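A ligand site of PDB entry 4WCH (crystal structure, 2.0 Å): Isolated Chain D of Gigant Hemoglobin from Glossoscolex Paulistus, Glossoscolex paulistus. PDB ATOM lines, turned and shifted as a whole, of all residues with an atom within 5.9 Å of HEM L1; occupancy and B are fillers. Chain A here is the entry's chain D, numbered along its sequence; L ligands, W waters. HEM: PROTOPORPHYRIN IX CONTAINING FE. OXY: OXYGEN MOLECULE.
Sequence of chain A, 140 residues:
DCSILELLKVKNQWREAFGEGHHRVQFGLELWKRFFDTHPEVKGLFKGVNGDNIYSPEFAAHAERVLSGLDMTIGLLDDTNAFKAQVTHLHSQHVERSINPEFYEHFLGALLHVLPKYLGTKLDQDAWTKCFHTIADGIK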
ATOM      1  N   TRP A  32     -19.363 -17.288 -20.172  1.00  0.00           N
ATOM      2  CA  TRP A  32     -19.869 -16.351 -19.169  1.00  0.00           C
ATOM      3  C   TRP A  32     -21.318 -16.638 -18.770  1.00  0.00           C
ATOM      4  O   TRP A  32     -21.722 -16.362 -17.646  1.00  0.00           O
ATOM      5  CB  TRP A  32     -19.708 -14.903 -19.652  1.00  0.00           C
ATOM      6  CG  TRP A  32     -18.282 -14.474 -19.589  1.00  0.00           C
ATOM      7  CD1 TRP A  32     -17.393 -14.389 -20.623  1.00  0.00           C
ATOM      8  CD2 TRP A  32     -17.559 -14.076 -18.414  1.00  0.00           C
ATOM      9  NE1 TRP A  32     -16.168 -13.962 -20.161  1.00  0.00           N
ATOM     10  CE2 TRP A  32     -16.240 -13.777 -18.813  1.00  0.00           C
ATOM     11  CE3 TRP A  32     -17.900 -13.978 -17.062  1.00  0.00           C
ATOM     12  CZ2 TRP A  32     -15.270 -13.353 -17.911  1.00  0.00           C
ATOM     13  CZ3 TRP A  32     -16.935 -13.554 -16.174  1.00  0.00           C
ATOM     14  CH2 TRP A  32     -15.639 -13.252 -16.602  1.00  0.00           C
ATOM     15  N   PHE A  35     -20.974 -19.509 -16.299  1.00  0.00           N
ATOM     16  CA  PHE A  35     -20.398 -18.983 -15.068  1.00  0.00           C
ATOM     17  C   PHE A  35     -21.459 -18.223 -14.267  1.00  0.00           C
ATOM     18  O   PHE A  35     -21.656 -18.476 -13.082  1.00  0.00           O
ATOM     19  CB  PHE A  35     -19.222 -18.062 -15.394  1.00  0.00           C
ATOM     20  CG  PHE A  35     -18.386 -17.677 -14.206  1.00  0.00           C
ATOM     21  CD1 PHE A  35     -18.381 -18.436 -13.047  1.00  0.00           C
ATOM     22  CD2 PHE A  35     -17.600 -16.541 -14.250  1.00  0.00           C
ATOM     23  CE1 PHE A  35     -17.599 -18.073 -11.975  1.00  0.00           C
ATOM     24  CE2 PHE A  35     -16.818 -16.177 -13.178  1.00  0.00           C
ATOM     25  CZ  PHE A  35     -16.818 -16.936 -12.033  1.00  0.00           C
ATOM     26  N   VAL A  42     -21.682 -13.599  -8.681  1.00  0.00           N
ATOM     27  CA  VAL A  42     -20.457 -13.006  -9.223  1.00  0.00           C
ATOM     28  C   VAL A  42     -20.739 -11.823 -10.148  1.00  0.00           C
ATOM     29  O   VAL A  42     -19.840 -11.026 -10.438  1.00  0.00           O
ATOM     30  CB  VAL A  42     -19.589 -14.067  -9.960  1.00  0.00           C
ATOM     31  CG1 VAL A  42     -20.175 -14.389 -11.333  1.00  0.00           C
ATOM     32  CG2 VAL A  42     -18.154 -13.573 -10.088  1.00  0.00           C
ATOM     33  N   LEU A  45     -19.692  -8.003  -9.698  1.00  0.00           N
ATOM     34  CA  LEU A  45     -18.348  -7.530 -10.011  1.00  0.00           C
ATOM     35  C   LEU A  45     -18.205  -6.995 -11.436  1.00  0.00           C
ATOM     36  O   LEU A  45     -17.165  -6.426 -11.787  1.00  0.00           O
ATOM     37  CB  LEU A  45     -17.346  -8.674  -9.814  1.00  0.00           C
ATOM     38  CG  LEU A  45     -17.173  -9.168  -8.380  1.00  0.00           C
ATOM     39  CD1 LEU A  45     -16.396 -10.473  -8.365  1.00  0.00           C
ATOM     40  CD2 LEU A  45     -16.468  -8.123  -7.527  1.00  0.00           C
ATOM     41  N   PHE A  46     -19.228  -7.168 -12.255  1.00  0.00           N
ATOM     42  CA  PHE A  46     -19.122  -6.844 -13.679  1.00  0.00           C
ATOM     43  C   PHE A  46     -20.041  -5.713 -14.144  1.00  0.00           C
ATOM     44  O   PHE A  46     -20.367  -5.626 -15.327  1.00  0.00           O
ATOM     45  CB  PHE A  46     -19.385  -8.106 -14.502  1.00  0.00           C
ATOM     46  CG  PHE A  46     -18.298  -9.151 -14.366  1.00  0.00           C
ATOM     47  CD1 PHE A  46     -17.158  -9.094 -15.142  1.00  0.00           C
ATOM     48  CD2 PHE A  46     -18.419 -10.188 -13.445  1.00  0.00           C
ATOM     49  CE1 PHE A  46     -16.155 -10.048 -15.007  1.00  0.00           C
ATOM     50  CE2 PHE A  46     -17.425 -11.146 -13.307  1.00  0.00           C
ATOM     51  CZ  PHE A  46     -16.290 -11.083 -14.089  1.00  0.00           C
ATOM     52  N   LYS A  47     -20.430  -4.828 -13.226  1.00  0.00           N
ATOM     53  CA  LYS A  47     -21.360  -3.748 -13.552  1.00  0.00           C
ATOM     54  C   LYS A  47     -20.737  -2.712 -14.475  1.00  0.00           C
ATOM     55  O   LYS A  47     -21.447  -1.997 -15.195  1.00  0.00           O
ATOM     56  CB  LYS A  47     -21.863  -3.055 -12.278  1.00  0.00           C
ATOM     57  CG  LYS A  47     -22.844  -3.883 -11.481  1.00  0.00           C
ATOM     58  CD  LYS A  47     -24.240  -3.839 -12.099  1.00  0.00           C
ATOM     59  CE  LYS A  47     -25.171  -4.865 -11.459  1.00  0.00           C
ATOM     60  NZ  LYS A  47     -25.291  -4.676  -9.983  1.00  0.00           N
ATOM     61  N   GLY A  48     -19.416  -2.614 -14.454  1.00  0.00           N
ATOM     62  CA  GLY A  48     -18.703  -1.689 -15.316  1.00  0.00           C
ATOM     63  C   GLY A  48     -18.727  -2.101 -16.785  1.00  0.00           C
ATOM     64  O   GLY A  48     -18.426  -1.297 -17.668  1.00  0.00           O
ATOM     65  N   VAL A  49     -19.095  -3.358 -17.026  1.00  0.00           N
ATOM     66  CA  VAL A  49     -19.176  -3.895 -18.384  1.00  0.00           C
ATOM     67  C   VAL A  49     -20.557  -4.506 -18.633  1.00  0.00           C
ATOM     68  O   VAL A  49     -20.720  -5.351 -19.518  1.00  0.00           O
ATOM     69  CB  VAL A  49     -18.093  -4.956 -18.635  1.00  0.00           C
ATOM     70  CG1 VAL A  49     -16.700  -4.328 -18.561  1.00  0.00           C
ATOM     71  CG2 VAL A  49     -18.223  -6.103 -17.642  1.00  0.00           C
ATOM     72  N   HIS A  62     -15.990  -7.008 -23.365  1.00  0.00           N
ATOM     73  CA  HIS A  62     -15.299  -7.548 -22.199  1.00  0.00           C
ATOM     74  C   HIS A  62     -14.957  -9.003 -22.436  1.00  0.00           C
ATOM     75  O   HIS A  62     -13.821  -9.422 -22.226  1.00  0.00           O
ATOM     76  CB  HIS A  62     -16.185  -7.420 -20.966  1.00  0.00           C
ATOM     77  CG  HIS A  62     -15.695  -8.211 -19.795  1.00  0.00           C
ATOM     78  ND1 HIS A  62     -14.672  -7.772 -18.986  1.00  0.00           N
ATOM     79  CD2 HIS A  62     -16.070  -9.413 -19.308  1.00  0.00           C
ATOM     80  CE1 HIS A  62     -14.445  -8.666 -18.037  1.00  0.00           C
ATOM     81  NE2 HIS A  62     -15.283  -9.674 -18.216  1.00  0.00           N
ATOM     82  N   ARG A  65     -12.098  -9.431 -24.699  1.00  0.00           N
ATOM     83  CA  ARG A  65     -10.856  -9.043 -24.041  1.00  0.00           C
ATOM     84  C   ARG A  65     -10.357 -10.184 -23.161  1.00  0.00           C
ATOM     85  O   ARG A  65      -9.144 -10.397 -23.039  1.00  0.00           O
ATOM     86  CB  ARG A  65     -11.063  -7.785 -23.197  1.00  0.00           C
ATOM     87  CG  ARG A  65     -11.258  -6.513 -24.026  1.00  0.00           C
ATOM     88  CD  ARG A  65     -10.986  -5.247 -23.206  1.00  0.00           C
ATOM     89  NE  ARG A  65     -11.991  -5.002 -22.173  1.00  0.00           N
ATOM     90  CZ  ARG A  65     -13.147  -4.394 -22.378  1.00  0.00           C
ATOM     91  NH1 ARG A  65     -13.499  -3.964 -23.586  1.00  0.00           N
ATOM     92  NH2 ARG A  65     -13.979  -4.213 -21.352  1.00  0.00           N
ATOM     93  N   VAL A  66     -11.281 -10.916 -22.542  1.00  0.00           N
ATOM     94  CA  VAL A  66     -10.900 -12.011 -21.652  1.00  0.00           C
ATOM     95  C   VAL A  66     -10.293 -13.172 -22.440  1.00  0.00           C
ATOM     96  O   VAL A  66      -9.275 -13.719 -22.038  1.00  0.00           O
ATOM     97  CB  VAL A  66     -12.102 -12.517 -20.811  1.00  0.00           C
ATOM     98  CG1 VAL A  66     -11.720 -13.789 -20.032  1.00  0.00           C
ATOM     99  CG2 VAL A  66     -12.593 -11.423 -19.868  1.00  0.00           C
ATOM    100  N   SER A  68      -8.795 -12.905 -25.258  1.00  0.00           N
ATOM    101  CA  SER A  68      -7.483 -12.462 -25.731  1.00  0.00           C
ATOM    102  C   SER A  68      -6.426 -12.642 -24.651  1.00  0.00           C
ATOM    103  O   SER A  68      -5.320 -13.098 -24.931  1.00  0.00           O
ATOM    104  CB  SER A  68      -7.524 -11.002 -26.189  1.00  0.00           C
ATOM    105  OG  SER A  68      -7.985 -10.916 -27.535  1.00  0.00           O
ATOM    106  N   GLY A  69      -6.774 -12.297 -23.412  1.00  0.00           N
ATOM    107  CA  GLY A  69      -5.847 -12.439 -22.302  1.00  0.00           C
ATOM    108  C   GLY A  69      -5.501 -13.904 -22.114  1.00  0.00           C
ATOM    109  O   GLY A  69      -4.348 -14.272 -21.895  1.00  0.00           O
ATOM    110  N   LEU A  70      -6.532 -14.729 -22.205  1.00  0.00           N
ATOM    111  CA  LEU A  70      -6.366 -16.174 -22.119  1.00  0.00           C
ATOM    112  C   LEU A  70      -5.431 -16.631 -23.246  1.00  0.00           C
ATOM    113  O   LEU A  70      -4.479 -17.374 -23.006  1.00  0.00           O
ATOM    114  CB  LEU A  70      -7.745 -16.828 -22.249  1.00  0.00           C
ATOM    115  CG  LEU A  70      -8.042 -18.148 -21.549  1.00  0.00           C
ATOM    116  CD1 LEU A  70      -7.478 -18.210 -20.142  1.00  0.00           C
ATOM    117  CD2 LEU A  70      -9.556 -18.340 -21.517  1.00  0.00           C
ATOM    118  N   THR A  73      -1.657 -15.567 -22.452  1.00  0.00           N
ATOM    119  CA  THR A  73      -0.995 -16.332 -21.408  1.00  0.00           C
ATOM    120  C   THR A  73      -0.759 -17.784 -21.811  1.00  0.00           C
ATOM    121  O   THR A  73       0.341 -18.307 -21.669  1.00  0.00           O
ATOM    122  CB  THR A  73      -1.762 -16.256 -20.059  1.00  0.00           C
ATOM    123  OG1 THR A  73      -3.112 -16.725 -20.246  1.00  0.00           O
ATOM    124  CG2 THR A  73      -1.782 -14.820 -19.544  1.00  0.00           C
ATOM    125  N   LEU A  90      -1.864  -8.883 -15.861  1.00  0.00           N
ATOM    126  CA  LEU A  90      -3.213  -9.336 -15.539  1.00  0.00           C
ATOM    127  C   LEU A  90      -3.507  -9.160 -14.055  1.00  0.00           C
ATOM    128  O   LEU A  90      -4.613  -8.784 -13.677  1.00  0.00           O
ATOM    129  CB  LEU A  90      -3.419 -10.794 -15.946  1.00  0.00           C
ATOM    130  CG  LEU A  90      -3.699 -11.058 -17.418  1.00  0.00           C
ATOM    131  CD1 LEU A  90      -3.759 -12.554 -17.680  1.00  0.00           C
ATOM    132  CD2 LEU A  90      -5.000 -10.385 -17.858  1.00  0.00           C
ATOM    133  N   GLN A  93      -4.657  -5.851 -13.170  1.00  0.00           N
ATOM    134  CA  GLN A  93      -5.990  -5.539 -13.677  1.00  0.00           C
ATOM    135  C   GLN A  93      -7.102  -6.205 -12.867  1.00  0.00           C
ATOM    136  O   GLN A  93      -8.287  -5.918 -13.081  1.00  0.00           O
ATOM    137  CB  GLN A  93      -6.077  -5.943 -15.154  1.00  0.00           C
ATOM    138  CG  GLN A  93      -5.201  -5.089 -16.057  1.00  0.00           C
ATOM    139  CD  GLN A  93      -5.103  -5.629 -17.462  1.00  0.00           C
ATOM    140  OE1 GLN A  93      -5.083  -6.842 -17.680  1.00  0.00           O
ATOM    141  NE2 GLN A  93      -5.057  -4.729 -18.438  1.00  0.00           N
ATOM    142  N   HIS A  94      -6.733  -7.061 -11.922  1.00  0.00           N
ATOM    143  CA  HIS A  94      -7.714  -7.749 -11.089  1.00  0.00           C
ATOM    144  C   HIS A  94      -7.584  -7.413  -9.604  1.00  0.00           C
ATOM    145  O   HIS A  94      -8.458  -7.760  -8.804  1.00  0.00           O
ATOM    146  CB  HIS A  94      -7.580  -9.264 -11.276  1.00  0.00           C
ATOM    147  CG  HIS A  94      -8.060  -9.766 -12.594  1.00  0.00           C
ATOM    148  ND1 HIS A  94      -7.374  -9.559 -13.769  1.00  0.00           N
ATOM    149  CD2 HIS A  94      -9.157 -10.480 -12.933  1.00  0.00           C
ATOM    150  CE1 HIS A  94      -8.027 -10.118 -14.772  1.00  0.00           C
ATOM    151  NE2 HIS A  94      -9.119 -10.693 -14.283  1.00  0.00           N
ATOM    152  N   ARG A  97     -10.232  -5.237  -7.126  1.00  0.00           N
ATOM    153  CA  ARG A  97     -11.628  -5.484  -7.471  1.00  0.00           C
ATOM    154  C   ARG A  97     -12.302  -6.431  -6.494  1.00  0.00           C
ATOM    155  O   ARG A  97     -13.444  -6.836  -6.694  1.00  0.00           O
ATOM    156  CB  ARG A  97     -11.722  -6.025  -8.906  1.00  0.00           C
ATOM    157  CG  ARG A  97     -11.257  -4.999  -9.931  1.00  0.00           C
ATOM    158  CD  ARG A  97     -11.408  -5.478 -11.356  1.00  0.00           C
ATOM    159  NE  ARG A  97     -11.022  -4.445 -12.308  1.00  0.00           N
ATOM    160  CZ  ARG A  97     -11.789  -3.415 -12.653  1.00  0.00           C
ATOM    161  NH1 ARG A  97     -12.993  -3.254 -12.126  1.00  0.00           N
ATOM    162  NH2 ARG A  97     -11.344  -2.520 -13.534  1.00  0.00           N
ATOM    163  N   ILE A  99     -11.969  -9.559  -5.723  1.00  0.00           N
ATOM    164  CA  ILE A  99     -12.384 -10.844  -6.261  1.00  0.00           C
ATOM    165  C   ILE A  99     -12.046 -11.931  -5.259  1.00  0.00           C
ATOM    166  O   ILE A  99     -10.875 -12.159  -4.951  1.00  0.00           O
ATOM    167  CB  ILE A  99     -11.699 -11.133  -7.610  1.00  0.00           C
ATOM    168  CG1 ILE A  99     -12.104 -10.069  -8.634  1.00  0.00           C
ATOM    169  CG2 ILE A  99     -12.098 -12.508  -8.108  1.00  0.00           C
ATOM    170  CD1 ILE A  99     -11.380 -10.193  -9.967  1.00  0.00           C
ATOM    171  N   ASN A 100     -13.068 -12.597  -4.741  1.00  0.00           N
ATOM    172  CA  ASN A 100     -12.846 -13.761  -3.900  1.00  0.00           C
ATOM    173  C   ASN A 100     -12.153 -14.831  -4.727  1.00  0.00           C
ATOM    174  O   ASN A 100     -12.677 -15.262  -5.761  1.00  0.00           O
ATOM    175  CB  ASN A 100     -14.176 -14.288  -3.352  1.00  0.00           C
ATOM    176  CG  ASN A 100     -13.991 -15.334  -2.283  1.00  0.00           C
ATOM    177  OD1 ASN A 100     -13.016 -16.082  -2.305  1.00  0.00           O
ATOM    178  ND2 ASN A 100     -14.914 -15.383  -1.335  1.00  0.00           N
ATOM    179  N   PHE A 103     -13.494 -17.845  -6.812  1.00  0.00           N
ATOM    180  CA  PHE A 103     -14.139 -17.616  -8.088  1.00  0.00           C
ATOM    181  C   PHE A 103     -13.325 -18.198  -9.254  1.00  0.00           C
ATOM    182  O   PHE A 103     -13.893 -18.657 -10.250  1.00  0.00           O
ATOM    183  CB  PHE A 103     -14.411 -16.128  -8.294  1.00  0.00           C
ATOM    184  CG  PHE A 103     -15.683 -15.649  -7.650  1.00  0.00           C
ATOM    185  CD1 PHE A 103     -16.858 -16.359  -7.820  1.00  0.00           C
ATOM    186  CD2 PHE A 103     -15.716 -14.501  -6.865  1.00  0.00           C
ATOM    187  CE1 PHE A 103     -18.039 -15.953  -7.229  1.00  0.00           C
ATOM    188  CE2 PHE A 103     -16.902 -14.082  -6.273  1.00  0.00           C
ATOM    189  CZ  PHE A 103     -18.055 -14.804  -6.458  1.00  0.00           C
ATOM    190  N   TYR A 104     -12.003 -18.210  -9.134  1.00  0.00           N
ATOM    191  CA  TYR A 104     -11.155 -18.720 -10.215  1.00  0.00           C
ATOM    192  C   TYR A 104     -11.394 -20.210 -10.461  1.00  0.00           C
ATOM    193  O   TYR A 104     -11.309 -20.675 -11.585  1.00  0.00           O
ATOM    194  CB  TYR A 104      -9.681 -18.457  -9.950  1.00  0.00           C
ATOM    195  CG  TYR A 104      -9.328 -17.002 -10.072  1.00  0.00           C
ATOM    196  CD1 TYR A 104      -9.076 -16.434 -11.310  1.00  0.00           C
ATOM    197  CD2 TYR A 104      -9.256 -16.188  -8.961  1.00  0.00           C
ATOM    198  CE1 TYR A 104      -8.764 -15.101 -11.433  1.00  0.00           C
ATOM    199  CE2 TYR A 104      -8.953 -14.852  -9.073  1.00  0.00           C
ATOM    200  CZ  TYR A 104      -8.700 -14.314 -10.311  1.00  0.00           C
ATOM    201  OH  TYR A 104      -8.397 -12.978 -10.423  1.00  0.00           O
ATOM    202  N   PHE A 107     -14.546 -20.325 -12.475  1.00  0.00           N
ATOM    203  CA  PHE A 107     -14.308 -19.913 -13.841  1.00  0.00           C
ATOM    204  C   PHE A 107     -13.771 -21.126 -14.597  1.00  0.00           C
ATOM    205  O   PHE A 107     -14.249 -21.458 -15.678  1.00  0.00           O
ATOM    206  CB  PHE A 107     -13.317 -18.752 -13.889  1.00  0.00           C
ATOM    207  CG  PHE A 107     -13.030 -18.229 -15.274  1.00  0.00           C
ATOM    208  CD1 PHE A 107     -13.706 -17.139 -15.777  1.00  0.00           C
ATOM    209  CD2 PHE A 107     -12.055 -18.819 -16.054  1.00  0.00           C
ATOM    210  CE1 PHE A 107     -13.430 -16.649 -17.038  1.00  0.00           C
ATOM    211  CE2 PHE A 107     -11.778 -18.329 -17.314  1.00  0.00           C
ATOM    212  CZ  PHE A 107     -12.459 -17.249 -17.809  1.00  0.00           C
ATOM    213  N   PHE A 132      -4.248 -24.023 -16.220  1.00  0.00           N
ATOM    214  CA  PHE A 132      -5.102 -22.931 -15.764  1.00  0.00           C
ATOM    215  C   PHE A 132      -4.689 -22.431 -14.379  1.00  0.00           C
ATOM    216  O   PHE A 132      -4.641 -21.219 -14.132  1.00  0.00           O
ATOM    217  CB  PHE A 132      -6.577 -23.352 -15.729  1.00  0.00           C
ATOM    218  CG  PHE A 132      -7.496 -22.279 -15.191  1.00  0.00           C
ATOM    219  CD1 PHE A 132      -8.120 -21.393 -16.047  1.00  0.00           C
ATOM    220  CD2 PHE A 132      -7.718 -22.160 -13.828  1.00  0.00           C
ATOM    221  CE1 PHE A 132      -8.957 -20.391 -15.551  1.00  0.00           C
ATOM    222  CE2 PHE A 132      -8.559 -21.168 -13.324  1.00  0.00           C
ATOM    223  CZ  PHE A 132      -9.178 -20.278 -14.197  1.00  0.00           C
ATOM    224  N   ILE A 135      -1.916 -20.081 -14.458  1.00  0.00           N
ATOM    225  CA  ILE A 135      -2.359 -18.766 -14.902  1.00  0.00           C
ATOM    226  C   ILE A 135      -3.071 -18.027 -13.781  1.00  0.00           C
ATOM    227  O   ILE A 135      -2.794 -16.853 -13.508  1.00  0.00           O
ATOM    228  CB  ILE A 135      -3.282 -18.867 -16.131  1.00  0.00           C
ATOM    229  CG1 ILE A 135      -2.496 -19.323 -17.356  1.00  0.00           C
ATOM    230  CG2 ILE A 135      -3.934 -17.513 -16.414  1.00  0.00           C
ATOM    231  CD1 ILE A 135      -3.364 -19.793 -18.509  1.00  0.00           C
ATOM    232  N   ALA A 136      -4.010 -18.716 -13.120  1.00  0.00           N
ATOM    233  CA  ALA A 136      -4.766 -18.136 -12.019  1.00  0.00           C
ATOM    234  C   ALA A 136      -3.855 -17.711 -10.865  1.00  0.00           C
ATOM    235  O   ALA A 136      -4.049 -16.652 -10.285  1.00  0.00           O
ATOM    236  CB  ALA A 136      -5.825 -19.116 -11.530  1.00  0.00           C
ATOM    237  N   ILE A 139      -2.384 -14.453 -11.820  1.00  0.00           N
ATOM    238  CA  ILE A 139      -3.345 -13.351 -11.724  1.00  0.00           C
ATOM    239  C   ILE A 139      -3.607 -12.953 -10.276  1.00  0.00           C
ATOM    240  O   ILE A 139      -3.665 -11.768  -9.940  1.00  0.00           O
ATOM    241  CB  ILE A 139      -4.687 -13.706 -12.401  1.00  0.00           C
ATOM    242  CG1 ILE A 139      -4.486 -13.792 -13.914  1.00  0.00           C
ATOM    243  CG2 ILE A 139      -5.746 -12.655 -12.061  1.00  0.00           C
ATOM    244  CD1 ILE A 139      -5.704 -14.249 -14.685  1.00  0.00           C
HETATM  245  CHA HEM L   1     -11.098  -7.835 -16.563  1.00  0.00           C
HETATM  246  CHB HEM L   1      -8.735 -11.755 -18.190  1.00  0.00           C
HETATM  247  CHC HEM L   1     -10.588 -14.405 -14.543  1.00  0.00           C
HETATM  248  CHD HEM L   1     -13.138 -10.565 -13.022  1.00  0.00           C
HETATM  249  C1A HEM L   1     -10.320  -8.659 -17.339  1.00  0.00           C
HETATM  250  C2A HEM L   1      -9.641  -8.295 -18.573  1.00  0.00           C
HETATM  251  C3A HEM L   1      -8.979  -9.371 -19.007  1.00  0.00           C
HETATM  252  C4A HEM L   1      -9.224 -10.469 -18.087  1.00  0.00           C
HETATM  253  CMA HEM L   1      -8.119  -9.427 -20.291  1.00  0.00           C
HETATM  254  CAA HEM L   1      -9.636  -6.906 -19.248  1.00  0.00           C
HETATM  255  CBA HEM L   1      -8.871  -5.909 -18.378  1.00  0.00           C
HETATM  256  CGA HEM L   1      -8.812  -4.542 -19.020  1.00  0.00           C
HETATM  257  O1A HEM L   1      -8.543  -4.439 -20.243  1.00  0.00           O
HETATM  258  O2A HEM L   1      -9.020  -3.543 -18.293  1.00  0.00           O
HETATM  259  C1B HEM L   1      -9.027 -12.801 -17.345  1.00  0.00           C
HETATM  260  C2B HEM L   1      -8.487 -14.142 -17.465  1.00  0.00           C
HETATM  261  C3B HEM L   1      -9.013 -14.884 -16.467  1.00  0.00           C
HETATM  262  C4B HEM L   1      -9.876 -14.027 -15.669  1.00  0.00           C
HETATM  263  CMB HEM L   1      -7.514 -14.555 -18.590  1.00  0.00           C
HETATM  264  CAB HEM L   1      -8.762 -16.373 -16.126  1.00  0.00           C
HETATM  265  CBB HEM L   1      -7.722 -17.058 -16.606  1.00  0.00           C
HETATM  266  C1C HEM L   1     -11.482 -13.615 -13.846  1.00  0.00           C
HETATM  267  C2C HEM L   1     -12.376 -14.047 -12.784  1.00  0.00           C
HETATM  268  C3C HEM L   1     -13.077 -12.986 -12.351  1.00  0.00           C
HETATM  269  C4C HEM L   1     -12.658 -11.845 -13.144  1.00  0.00           C
HETATM  270  CMC HEM L   1     -12.425 -15.501 -12.280  1.00  0.00           C
HETATM  271  CAC HEM L   1     -14.161 -12.854 -11.259  1.00  0.00           C
HETATM  272  CBC HEM L   1     -14.721 -13.897 -10.651  1.00  0.00           C
HETATM  273  C1D HEM L   1     -12.801  -9.488 -13.801  1.00  0.00           C
HETATM  274  C2D HEM L   1     -13.322  -8.156 -13.605  1.00  0.00           C
HETATM  275  C3D HEM L   1     -12.690  -7.294 -14.708  1.00  0.00           C
HETATM  276  C4D HEM L   1     -11.847  -8.202 -15.462  1.00  0.00           C
HETATM  277  CMD HEM L   1     -14.307  -7.684 -12.507  1.00  0.00           C
HETATM  278  CAD HEM L   1     -12.905  -5.787 -14.957  1.00  0.00           C
HETATM  279  CBD HEM L   1     -14.268  -5.545 -15.603  1.00  0.00           C
HETATM  280  CGD HEM L   1     -14.437  -4.070 -15.823  1.00  0.00           C
HETATM  281  O1D HEM L   1     -13.818  -3.548 -16.783  1.00  0.00           O
HETATM  282  O2D HEM L   1     -15.181  -3.425 -15.034  1.00  0.00           O
HETATM  283  NA  HEM L   1     -10.049  -9.994 -17.082  1.00  0.00           N
HETATM  284  NB  HEM L   1      -9.853 -12.764 -16.244  1.00  0.00           N
HETATM  285  NC  HEM L   1     -11.695 -12.258 -14.041  1.00  0.00           N
HETATM  286  ND  HEM L   1     -11.941  -9.474 -14.907  1.00  0.00           N
HETATM  287 FE   HEM L   1     -10.810 -11.116 -15.549  1.00  0.00          FE
HETATM  288  O1  OXY L   2     -12.231 -11.580 -16.519  1.00  0.00           O
HETATM  289  O2  OXY L   2     -13.572 -11.233 -16.000  1.00  0.00           O
HETATM  290  O   HOH W   1      -7.076  -8.826 -23.457  1.00  0.00           O
HETATM  291  O   HOH W   2     -15.036  -0.889 -14.558  1.00  0.00           O
HETATM  292  O   HOH W   3      -7.501  -1.389 -18.317  1.00  0.00           O
HETATM  293  O   HOH W   4     -17.319  -4.297 -13.432  1.00  0.00           O
HETATM  294  O   HOH W   5     -12.840  -5.134 -18.578  1.00  0.00           O
HETATM  295  O   HOH W   6     -14.222  -1.190 -17.567  1.00  0.00           O
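An oxygen (O1) of OXY L2 is bound to an iron atom (FE) of HEM L1 (1.8 Å).
Water W5 lies within hydrogen-bond range of an oxygen (O1D) of HEM L1 (2.6 Å), the guanidinium group of Arg 65 (3.1 Å) and a ring nitrogen (ND1) of His 62 (3.2 Å).
Water W4 lies within hydrogen-bond range of the backbone carbonyl oxygen (O) of Leu 45, an oxygen (O2D) of HEM L1, the backbone NH (N) of Gly 48 and the backbone NH (N) of Lys 47.
The guanidinium group (NH1) of Arg 97 lies within salt-bridge range of an oxygen (O2D) of HEM L1 (3.6 Å).
NE2 of His 62 sits at hydrogen-bond distance from O2 of OXY L2, at 3.2 Å.
An iron atom (FE) of HEM L1 is bound by a ring nitrogen (NE2) of His 94, at 2.2 Å.
The guanidinium group of Arg 65 is in salt-bridge range of an oxygen (O1A) of HEM L1 (3.99 Å).
Residues that only touch HEM L1: Phe 35 (3.9 Å), Val 42 (3.5 Å), Leu 45 (3.2 Å), Phe 46 (3.4 Å), Gly 48 (3.9 Å), Val 49 (3.5 Å), His 62 (3.7 Å), Val 66 (3.9 Å), Leu 70 (3.7 Å), Leu 90 (3.99 Å), Gln 93 (3.8 Å), Ile 99 (3.5 Å), Phe 103 (3.3 Å), Tyr 104 (3.6 Å), Phe 107 (3.7 Å), Phe 132 (3.7 Å), Ile 135 (3.8 Å) and Ile 139 (3.8 Å).
Hydrophobic or aromatic side chains within 4 Å of HEM L1: Phe 35, Val 42, Phe 46, Val 49, His 62, Val 66, Leu 70, Leu 90, His 94, Ile 99, Phe 103, Tyr 104, Phe 107, Phe 132, Ile 135 and Ile 139.
The nearest printed residue that does not touch HEM L1 is Gly 69 (4.1 Å).
The guanidinium group (NE) of Arg 97 sits at hydrogen-bond distance from the backbone carbonyl oxygen (O) of Gln 93, 3.2 Å away.
The side-chain hydroxyl of Thr 73 sits at hydrogen-bond distance from the backbone carbonyl oxygen of Leu 70, at 3.1 Å.
A ring nitrogen (ND1) of His 94 lies within hydrogen-bond range of the backbone carbonyl oxygen (O) of Leu 90, at 2.9 Å.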
